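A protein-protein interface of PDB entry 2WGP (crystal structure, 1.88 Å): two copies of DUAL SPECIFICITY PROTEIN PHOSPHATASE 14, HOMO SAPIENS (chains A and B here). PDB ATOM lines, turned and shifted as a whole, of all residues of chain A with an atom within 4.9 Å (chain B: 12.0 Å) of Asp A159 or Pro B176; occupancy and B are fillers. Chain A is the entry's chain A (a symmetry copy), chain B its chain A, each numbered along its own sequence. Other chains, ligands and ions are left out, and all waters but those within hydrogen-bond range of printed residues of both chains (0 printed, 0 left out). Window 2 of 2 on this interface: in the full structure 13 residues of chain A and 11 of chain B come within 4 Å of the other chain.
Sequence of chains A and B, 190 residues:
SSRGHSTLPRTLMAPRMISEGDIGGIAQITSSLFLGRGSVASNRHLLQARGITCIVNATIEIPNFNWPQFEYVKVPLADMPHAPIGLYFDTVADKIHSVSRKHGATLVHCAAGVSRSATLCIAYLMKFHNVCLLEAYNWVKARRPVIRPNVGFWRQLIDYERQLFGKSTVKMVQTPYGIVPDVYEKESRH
NE2 of Gln A163 sits at hydrogen-bond distance from OH of Tyr B177.
The side-chain hydroxyl (OG1) of Thr B175 lies close to the backbone NH (N) of Tyr B177. The side-chain amide nitrogen of Gln A163 is in hydrogen-bond range of the side-chain carboxylate of Asp A159 (2.7 Å).
CB of Tyr B177 touches OE1 of Gln A156 (3.3 Å). OD1 of Asp A159 touches CB of Pro B176 (3.4 Å). CD1 of Tyr A160 touches OH of Tyr B177, 3.5 Å away.
Of chain B, only Pro B176 comes within 4 Å of Asp A159. Pro B176 touches just one residue of chain A: Asp A159. No residue of chain B comes within 4 Å of Ile A158. No residue of chain B comes within 4 Å of Arg A162. Of chain B, only Tyr B177 (2.8 Å) comes within 4 Å of Gln A163. Printed residues of chain B within 4 Å of Tyr A160: Tyr B177. Of the printed residues of chain A, Tyr B177 touches Gln A156 (3.3 Å), Tyr A160 (3.5 Å) and Gln A163 (2.8 Å). Pro B181 touches none of the printed residues of chain A. The nearest residue of chain A that does not touch Pro B176 is Gln A163 (4.3 Å).
Of the 9 printed residues of chain A, 4 touch a printed residue of chain B. Hydrophobic or aromatic side chains of chain A that line the printed part of chain B: Tyr A160. Among the printed residues, no Asp or Glu carboxylate lies within 4 Å of a Lys or Arg side-chain nitrogen of the other chain.
No position is printed for both chains. Of the 4 pairs that touch across the chains among the printed residues, none has its exchanged pair printed and touching as well.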
ATOM      1  N   ARG A 155       8.890 -12.237  16.000  1.00  0.00           N
ATOM      2  CA  ARG A 155       8.287 -12.649  17.294  1.00  0.00           C
ATOM      3  C   ARG A 155       8.514 -11.573  18.365  1.00  0.00           C
ATOM      4  O   ARG A 155       7.600 -11.195  19.086  1.00  0.00           O
ATOM      5  CB  ARG A 155       8.834 -13.990  17.792  1.00  0.00           C
ATOM      6  CG  ARG A 155       8.440 -15.175  16.951  1.00  0.00           C
ATOM      7  CD  ARG A 155       8.756 -16.508  17.648  1.00  0.00           C
ATOM      8  NE  ARG A 155      10.191 -16.785  17.796  1.00  0.00           N
ATOM      9  CZ  ARG A 155      10.985 -17.374  16.889  1.00  0.00           C
ATOM     10  NH1 ARG A 155      10.521 -17.757  15.699  1.00  0.00           N
ATOM     11  NH2 ARG A 155      12.266 -17.566  17.182  1.00  0.00           N
ATOM     12  N   GLN A 156       9.720 -11.034  18.398  1.00  0.00           N
ATOM     13  CA  GLN A 156      10.081 -10.061  19.420  1.00  0.00           C
ATOM     14  C   GLN A 156       9.395  -8.724  19.179  1.00  0.00           C
ATOM     15  O   GLN A 156       8.906  -8.096  20.124  1.00  0.00           O
ATOM     16  CB  GLN A 156      11.607  -9.929  19.507  1.00  0.00           C
ATOM     17  CG  GLN A 156      12.307 -11.208  19.977  1.00  0.00           C
ATOM     18  CD  GLN A 156      13.816 -11.087  20.052  1.00  0.00           C
ATOM     19  OE1 GLN A 156      14.339 -10.176  20.706  1.00  0.00           O
ATOM     20  NE2 GLN A 156      14.537 -12.036  19.422  1.00  0.00           N
ATOM     21  N   LEU A 157       9.339  -8.284  17.914  1.00  0.00           N
ATOM     22  CA  LEU A 157       8.593  -7.062  17.554  1.00  0.00           C
ATOM     23  C   LEU A 157       7.105  -7.149  17.898  1.00  0.00           C
ATOM     24  O   LEU A 157       6.506  -6.161  18.335  1.00  0.00           O
ATOM     25  CB  LEU A 157       8.726  -6.773  16.050  1.00  0.00           C
ATOM     26  CG  LEU A 157      10.055  -6.168  15.606  1.00  0.00           C
ATOM     27  CD1 LEU A 157      10.161  -6.204  14.110  1.00  0.00           C
ATOM     28  CD2 LEU A 157      10.258  -4.757  16.174  1.00  0.00           C
ATOM     29  N   ILE A 158       6.518  -8.323  17.674  1.00  0.00           N
ATOM     30  CA  ILE A 158       5.091  -8.564  17.939  1.00  0.00           C
ATOM     31  C   ILE A 158       4.804  -8.462  19.436  1.00  0.00           C
ATOM     32  O   ILE A 158       3.819  -7.854  19.837  1.00  0.00           O
ATOM     33  CB  ILE A 158       4.595  -9.924  17.385  1.00  0.00           C
ATOM     34  CG1 ILE A 158       4.483  -9.871  15.858  1.00  0.00           C
ATOM     35  CG2 ILE A 158       3.207 -10.284  18.006  1.00  0.00           C
ATOM     36  CD1 ILE A 158       4.428 -11.265  15.132  1.00  0.00           C
ATOM     37  N   ASP A 159       5.678  -9.055  20.252  1.00  0.00           N
ATOM     38  CA  ASP A 159       5.577  -8.914  21.710  1.00  0.00           C
ATOM     39  C   ASP A 159       5.680  -7.451  22.131  1.00  0.00           C
ATOM     40  O   ASP A 159       4.881  -6.996  22.931  1.00  0.00           O
ATOM     41  CB  ASP A 159       6.632  -9.772  22.447  1.00  0.00           C
ATOM     42  CG  ASP A 159       6.355  -9.858  23.947  1.00  0.00           C
ATOM     43  OD1 ASP A 159       6.651  -8.884  24.661  1.00  0.00           O
ATOM     44  OD2 ASP A 159       5.818 -10.885  24.414  1.00  0.00           O
ATOM     45  N   TYR A 160       6.650  -6.724  21.580  1.00  0.00           N
ATOM     46  CA  TYR A 160       6.862  -5.306  21.911  1.00  0.00           C
ATOM     47  C   TYR A 160       5.667  -4.450  21.497  1.00  0.00           C
ATOM     48  O   TYR A 160       5.227  -3.587  22.259  1.00  0.00           O
ATOM     49  CB  TYR A 160       8.121  -4.794  21.233  1.00  0.00           C
ATOM     50  CG  TYR A 160       8.604  -3.423  21.669  1.00  0.00           C
ATOM     51  CD1 TYR A 160       8.885  -3.146  23.020  1.00  0.00           C
ATOM     52  CD2 TYR A 160       8.837  -2.419  20.724  1.00  0.00           C
ATOM     53  CE1 TYR A 160       9.377  -1.918  23.412  1.00  0.00           C
ATOM     54  CE2 TYR A 160       9.298  -1.173  21.110  1.00  0.00           C
ATOM     55  CZ  TYR A 160       9.574  -0.934  22.453  1.00  0.00           C
ATOM     56  OH  TYR A 160      10.065   0.286  22.793  1.00  0.00           O
ATOM     57  N   GLU A 161       5.122  -4.725  20.307  1.00  0.00           N
ATOM     58  CA  GLU A 161       3.889  -4.062  19.866  1.00  0.00           C
ATOM     59  C   GLU A 161       2.754  -4.280  20.868  1.00  0.00           C
ATOM     60  O   GLU A 161       2.041  -3.337  21.222  1.00  0.00           O
ATOM     61  CB  GLU A 161       3.448  -4.556  18.500  1.00  0.00           C
ATOM     62  CG  GLU A 161       2.223  -3.735  17.968  1.00  0.00           C
ATOM     63  CD  GLU A 161       1.562  -4.293  16.731  1.00  0.00           C
ATOM     64  OE1 GLU A 161       1.696  -5.499  16.452  1.00  0.00           O
ATOM     65  OE2 GLU A 161       0.891  -3.487  16.015  1.00  0.00           O
ATOM     66  N   ARG A 162       2.593  -5.524  21.327  1.00  0.00           N
ATOM     67  CA  ARG A 162       1.549  -5.854  22.303  1.00  0.00           C
ATOM     68  C   ARG A 162       1.769  -5.110  23.625  1.00  0.00           C
ATOM     69  O   ARG A 162       0.800  -4.653  24.246  1.00  0.00           O
ATOM     70  CB  ARG A 162       1.466  -7.367  22.558  1.00  0.00           C
ATOM     71  CG  ARG A 162       0.940  -8.227  21.386  1.00  0.00           C
ATOM     72  CD  ARG A 162       1.188  -9.751  21.658  1.00  0.00           C
ATOM     73  NE  ARG A 162       0.274 -10.251  22.702  1.00  0.00           N
ATOM     74  CZ  ARG A 162       0.596 -11.053  23.727  1.00  0.00           C
ATOM     75  NH1 ARG A 162       1.833 -11.498  23.912  1.00  0.00           N
ATOM     76  NH2 ARG A 162      -0.342 -11.409  24.581  1.00  0.00           N
ATOM     77  N   GLN A 163       3.032  -4.990  24.052  1.00  0.00           N
ATOM     78  CA  GLN A 163       3.377  -4.225  25.258  1.00  0.00           C
ATOM     79  C   GLN A 163       2.976  -2.734  25.085  1.00  0.00           C
ATOM     80  O   GLN A 163       2.444  -2.099  25.998  1.00  0.00           O
ATOM     81  CB  GLN A 163       4.881  -4.295  25.552  1.00  0.00           C
ATOM     82  CG  GLN A 163       5.443  -5.657  25.925  1.00  0.00           C
ATOM     83  CD  GLN A 163       6.978  -5.624  26.037  1.00  0.00           C
ATOM     84  OE1 GLN A 163       7.513  -4.780  26.750  1.00  0.00           O
ATOM     85  NE2 GLN A 163       7.677  -6.493  25.287  1.00  0.00           N
ATOM     86  N   ARG B 148      29.859  -9.044  25.488  1.00  0.00           N
ATOM     87  CA  ARG B 148      28.522  -9.643  25.436  1.00  0.00           C
ATOM     88  C   ARG B 148      28.633 -11.147  25.125  1.00  0.00           C
ATOM     89  O   ARG B 148      28.335 -11.591  24.028  1.00  0.00           O
ATOM     90  CB  ARG B 148      27.683  -8.929  24.372  1.00  0.00           C
ATOM     91  CG  ARG B 148      26.217  -9.229  24.438  1.00  0.00           C
ATOM     92  CD  ARG B 148      25.484  -8.280  25.309  1.00  0.00           C
ATOM     93  NE  ARG B 148      24.052  -8.502  25.267  1.00  0.00           N
ATOM     94  CZ  ARG B 148      23.156  -7.835  25.990  1.00  0.00           C
ATOM     95  NH1 ARG B 148      23.549  -6.932  26.863  1.00  0.00           N
ATOM     96  NH2 ARG B 148      21.853  -8.085  25.824  1.00  0.00           N
ATOM     97  N   VAL B 151      24.489 -16.469  25.113  1.00  0.00           N
ATOM     98  CA  VAL B 151      23.753 -17.039  26.268  1.00  0.00           C
ATOM     99  C   VAL B 151      24.225 -18.432  26.701  1.00  0.00           C
ATOM    100  O   VAL B 151      24.144 -18.758  27.896  1.00  0.00           O
ATOM    101  CB  VAL B 151      22.226 -17.014  26.078  1.00  0.00           C
ATOM    102  CG1 VAL B 151      21.753 -15.532  26.033  1.00  0.00           C
ATOM    103  CG2 VAL B 151      21.813 -17.828  24.833  1.00  0.00           C
ATOM    104  N   MET B 172      20.068 -17.321  34.899  1.00  0.00           N
ATOM    105  CA  MET B 172      19.406 -17.214  33.596  1.00  0.00           C
ATOM    106  C   MET B 172      17.913 -16.999  33.861  1.00  0.00           C
ATOM    107  O   MET B 172      17.299 -17.699  34.671  1.00  0.00           O
ATOM    108  CB  MET B 172      19.667 -18.462  32.752  1.00  0.00           C
ATOM    109  CG  MET B 172      21.155 -18.752  32.533  1.00  0.00           C
ATOM    110  SD  MET B 172      22.076 -17.509  31.602  1.00  0.00           S
ATOM    111  CE  MET B 172      21.341 -17.617  30.002  1.00  0.00           C
ATOM    112  N   VAL B 173      17.360 -15.998  33.189  1.00  0.00           N
ATOM    113  CA  VAL B 173      15.973 -15.609  33.356  1.00  0.00           C
ATOM    114  C   VAL B 173      15.303 -15.498  31.985  1.00  0.00           C
ATOM    115  O   VAL B 173      15.944 -15.146  30.991  1.00  0.00           O
ATOM    116  CB  VAL B 173      15.835 -14.291  34.158  1.00  0.00           C
ATOM    117  CG1 VAL B 173      16.433 -14.461  35.611  1.00  0.00           C
ATOM    118  CG2 VAL B 173      16.452 -13.107  33.402  1.00  0.00           C
ATOM    119  N   GLN B 174      14.021 -15.851  31.947  1.00  0.00           N
ATOM    120  CA  GLN B 174      13.237 -15.779  30.745  1.00  0.00           C
ATOM    121  C   GLN B 174      12.647 -14.387  30.601  1.00  0.00           C
ATOM    122  O   GLN B 174      11.964 -13.888  31.507  1.00  0.00           O
ATOM    123  CB  GLN B 174      12.095 -16.791  30.790  1.00  0.00           C
ATOM    124  CG  GLN B 174      11.153 -16.688  29.606  1.00  0.00           C
ATOM    125  CD  GLN B 174      11.782 -17.218  28.365  1.00  0.00           C
ATOM    126  OE1 GLN B 174      12.139 -18.393  28.311  1.00  0.00           O
ATOM    127  NE2 GLN B 174      11.949 -16.363  27.357  1.00  0.00           N
ATOM    128  N   THR B 175      12.898 -13.782  29.450  1.00  0.00           N
ATOM    129  CA  THR B 175      12.332 -12.490  29.107  1.00  0.00           C
ATOM    130  C   THR B 175      11.484 -12.713  27.861  1.00  0.00           C
ATOM    131  O   THR B 175      11.549 -13.792  27.256  1.00  0.00           O
ATOM    132  CB  THR B 175      13.425 -11.423  28.843  1.00  0.00           C
ATOM    133  OG1 THR B 175      13.941 -11.573  27.516  1.00  0.00           O
ATOM    134  CG2 THR B 175      14.561 -11.514  29.864  1.00  0.00           C
ATOM    135  N   PRO B 176      10.700 -11.699  27.459  1.00  0.00           N
ATOM    136  CA  PRO B 176       9.961 -11.787  26.207  1.00  0.00           C
ATOM    137  C   PRO B 176      10.864 -12.015  24.993  1.00  0.00           C
ATOM    138  O   PRO B 176      10.381 -12.454  23.959  1.00  0.00           O
ATOM    139  CB  PRO B 176       9.268 -10.423  26.125  1.00  0.00           C
ATOM    140  CG  PRO B 176       9.240  -9.930  27.499  1.00  0.00           C
ATOM    141  CD  PRO B 176      10.458 -10.412  28.132  1.00  0.00           C
ATOM    142  N   TYR B 177      12.168 -11.758  25.128  1.00  0.00           N
ATOM    143  CA  TYR B 177      13.109 -11.810  24.010  1.00  0.00           C
ATOM    144  C   TYR B 177      14.053 -13.010  24.053  1.00  0.00           C
ATOM    145  O   TYR B 177      14.979 -13.098  23.266  1.00  0.00           O
ATOM    146  CB  TYR B 177      13.882 -10.481  23.976  1.00  0.00           C
ATOM    147  CG  TYR B 177      12.950  -9.295  24.088  1.00  0.00           C
ATOM    148  CD1 TYR B 177      11.837  -9.187  23.260  1.00  0.00           C
ATOM    149  CD2 TYR B 177      13.154  -8.289  25.034  1.00  0.00           C
ATOM    150  CE1 TYR B 177      10.957  -8.138  23.366  1.00  0.00           C
ATOM    151  CE2 TYR B 177      12.276  -7.214  25.138  1.00  0.00           C
ATOM    152  CZ  TYR B 177      11.182  -7.135  24.287  1.00  0.00           C
ATOM    153  OH  TYR B 177      10.277  -6.100  24.348  1.00  0.00           O
ATOM    154  N   GLY B 178      13.799 -13.926  24.987  1.00  0.00           N
ATOM    155  CA  GLY B 178      14.624 -15.085  25.199  1.00  0.00           C
ATOM    156  C   GLY B 178      15.151 -15.202  26.626  1.00  0.00           C
ATOM    157  O   GLY B 178      15.004 -14.299  27.464  1.00  0.00           O
ATOM    158  N   ILE B 179      15.763 -16.345  26.884  1.00  0.00           N
ATOM    159  CA  ILE B 179      16.412 -16.621  28.149  1.00  0.00           C
ATOM    160  C   ILE B 179      17.784 -15.963  28.105  1.00  0.00           C
ATOM    161  O   ILE B 179      18.549 -16.175  27.166  1.00  0.00           O
ATOM    162  CB  ILE B 179      16.539 -18.128  28.404  1.00  0.00           C
ATOM    163  CG1 ILE B 179      15.143 -18.745  28.591  1.00  0.00           C
ATOM    164  CG2 ILE B 179      17.403 -18.397  29.664  1.00  0.00           C
ATOM    165  CD1 ILE B 179      15.030 -20.246  28.247  1.00  0.00           C
ATOM    166  N   VAL B 180      18.101 -15.167  29.121  1.00  0.00           N
ATOM    167  CA  VAL B 180      19.370 -14.443  29.161  1.00  0.00           C
ATOM    168  C   VAL B 180      19.858 -14.396  30.601  1.00  0.00           C
ATOM    169  O   VAL B 180      19.036 -14.500  31.528  1.00  0.00           O
ATOM    170  CB  VAL B 180      19.198 -12.978  28.624  1.00  0.00           C
ATOM    171  CG1 VAL B 180      18.866 -12.989  27.132  1.00  0.00           C
ATOM    172  CG2 VAL B 180      18.098 -12.191  29.458  1.00  0.00           C
ATOM    173  N   PRO B 181      21.171 -14.178  30.806  1.00  0.00           N
ATOM    174  CA  PRO B 181      21.571 -13.867  32.168  1.00  0.00           C
ATOM    175  C   PRO B 181      20.832 -12.626  32.696  1.00  0.00           C
ATOM    176  O   PRO B 181      20.583 -11.654  31.950  1.00  0.00           O
ATOM    177  CB  PRO B 181      23.076 -13.600  32.054  1.00  0.00           C
ATOM    178  CG  PRO B 181      23.259 -13.161  30.609  1.00  0.00           C
ATOM    179  CD  PRO B 181      22.274 -13.990  29.842  1.00  0.00           C
ATOM    180  N   ASP B 182      20.519 -12.646  33.986  1.00  0.00           N
ATOM    181  CA  ASP B 182      19.821 -11.508  34.605  1.00  0.00           C
ATOM    182  C   ASP B 182      20.477 -10.141  34.370  1.00  0.00           C
ATOM    183  O   ASP B 182      19.766  -9.140  34.267  1.00  0.00           O
ATOM    184  CB  ASP B 182      19.485 -11.738  36.094  1.00  0.00           C
ATOM    185  CG  ASP B 182      20.668 -12.188  36.951  1.00  0.00           C
ATOM    186  OD1 ASP B 182      21.841 -11.908  36.648  1.00  0.00           O
ATOM    187  OD2 ASP B 182      20.396 -12.804  38.002  1.00  0.00           O
ATOM    188  N   TYR B 184      21.750  -8.954  31.672  1.00  0.00           N
ATOM    189  CA  TYR B 184      21.276  -8.410  30.392  1.00  0.00           C
ATOM    190  C   TYR B 184      19.869  -7.836  30.539  1.00  0.00           C
ATOM    191  O   TYR B 184      19.543  -6.814  29.945  1.00  0.00           O
ATOM    192  CB  TYR B 184      21.261  -9.470  29.300  1.00  0.00           C
ATOM    193  CG  TYR B 184      22.623  -9.909  28.773  1.00  0.00           C
ATOM    194  CD1 TYR B 184      23.822  -9.398  29.290  1.00  0.00           C
ATOM    195  CD2 TYR B 184      22.702 -10.863  27.755  1.00  0.00           C
ATOM    196  CE1 TYR B 184      25.041  -9.828  28.815  1.00  0.00           C
ATOM    197  CE2 TYR B 184      23.895 -11.299  27.276  1.00  0.00           C
ATOM    198  CZ  TYR B 184      25.082 -10.785  27.808  1.00  0.00           C
ATOM    199  OH  TYR B 184      26.303 -11.202  27.319  1.00  0.00           O
ATOM    200  N   GLU B 185      19.030  -8.511  31.317  1.00  0.00           N
ATOM    201  CA  GLU B 185      17.671  -8.008  31.558  1.00  0.00           C
ATOM    202  C   GLU B 185      17.766  -6.682  32.326  1.00  0.00           C
ATOM    203  O   GLU B 185      17.086  -5.712  31.988  1.00  0.00           O
ATOM    204  CB  GLU B 185      16.865  -9.052  32.327  1.00  0.00           C
ATOM    205  CG  GLU B 185      15.370  -8.900  32.219  1.00  0.00           C
ATOM    206  CD  GLU B 185      14.806  -7.930  33.230  1.00  0.00           C
ATOM    207  OE1 GLU B 185      15.501  -7.690  34.241  1.00  0.00           O
ATOM    208  OE2 GLU B 185      13.663  -7.435  33.035  1.00  0.00           O
ATOM    209  N   LYS B 186      18.602  -6.655  33.363  1.00  0.00           N
ATOM    210  CA  LYS B 186      18.804  -5.447  34.167  1.00  0.00           C
ATOM    211  C   LYS B 186      19.297  -4.260  33.321  1.00  0.00           C
ATOM    212  O   LYS B 186      18.770  -3.159  33.449  1.00  0.00           O
ATOM    213  CB  LYS B 186      19.719  -5.739  35.361  1.00  0.00           C
ATOM    214  CG  LYS B 186      19.069  -6.692  36.374  1.00  0.00           C
ATOM    215  CD  LYS B 186      20.017  -7.168  37.458  1.00  0.00           C
ATOM    216  CE  LYS B 186      19.265  -7.936  38.523  1.00  0.00           C
ATOM    217  NZ  LYS B 186      20.088  -8.133  39.744  1.00  0.00           N
ATOM    218  N   SER B 188      18.758  -3.752  30.165  1.00  0.00           N
ATOM    219  CA  SER B 188      17.681  -3.374  29.216  1.00  0.00           C
ATOM    220  C   SER B 188      16.692  -2.354  29.796  1.00  0.00           C
ATOM    221  O   SER B 188      15.957  -1.696  29.053  1.00  0.00           O
ATOM    222  CB  SER B 188      16.893  -4.602  28.727  1.00  0.00           C
ATOM    223  OG  SER B 188      16.006  -5.109  29.717  1.00  0.00           O
ATOM    224  N   ARG B 189      16.683  -2.257  31.119  1.00  0.00           N
ATOM    225  CA  ARG B 189      15.833  -1.331  31.844  1.00  0.00           C
ATOM    226  C   ARG B 189      16.646  -0.124  32.318  1.00  0.00           C
ATOM    227  O   ARG B 189      16.165   0.663  33.111  1.00  0.00           O
ATOM    228  CB  ARG B 189      15.227  -2.062  33.041  1.00  0.00           C
ATOM    229  CG  ARG B 189      14.395  -3.290  32.655  1.00  0.00           C
ATOM    230  CD  ARG B 189      14.473  -4.350  33.723  1.00  0.00           C
ATOM    231  NE  ARG B 189      14.306  -3.760  35.049  1.00  0.00           N
ATOM    232  CZ  ARG B 189      14.903  -4.178  36.164  1.00  0.00           C
ATOM    233  NH1 ARG B 189      15.735  -5.218  36.161  1.00  0.00           N
ATOM    234  NH2 ARG B 189      14.666  -3.536  37.302  1.00  0.00           N
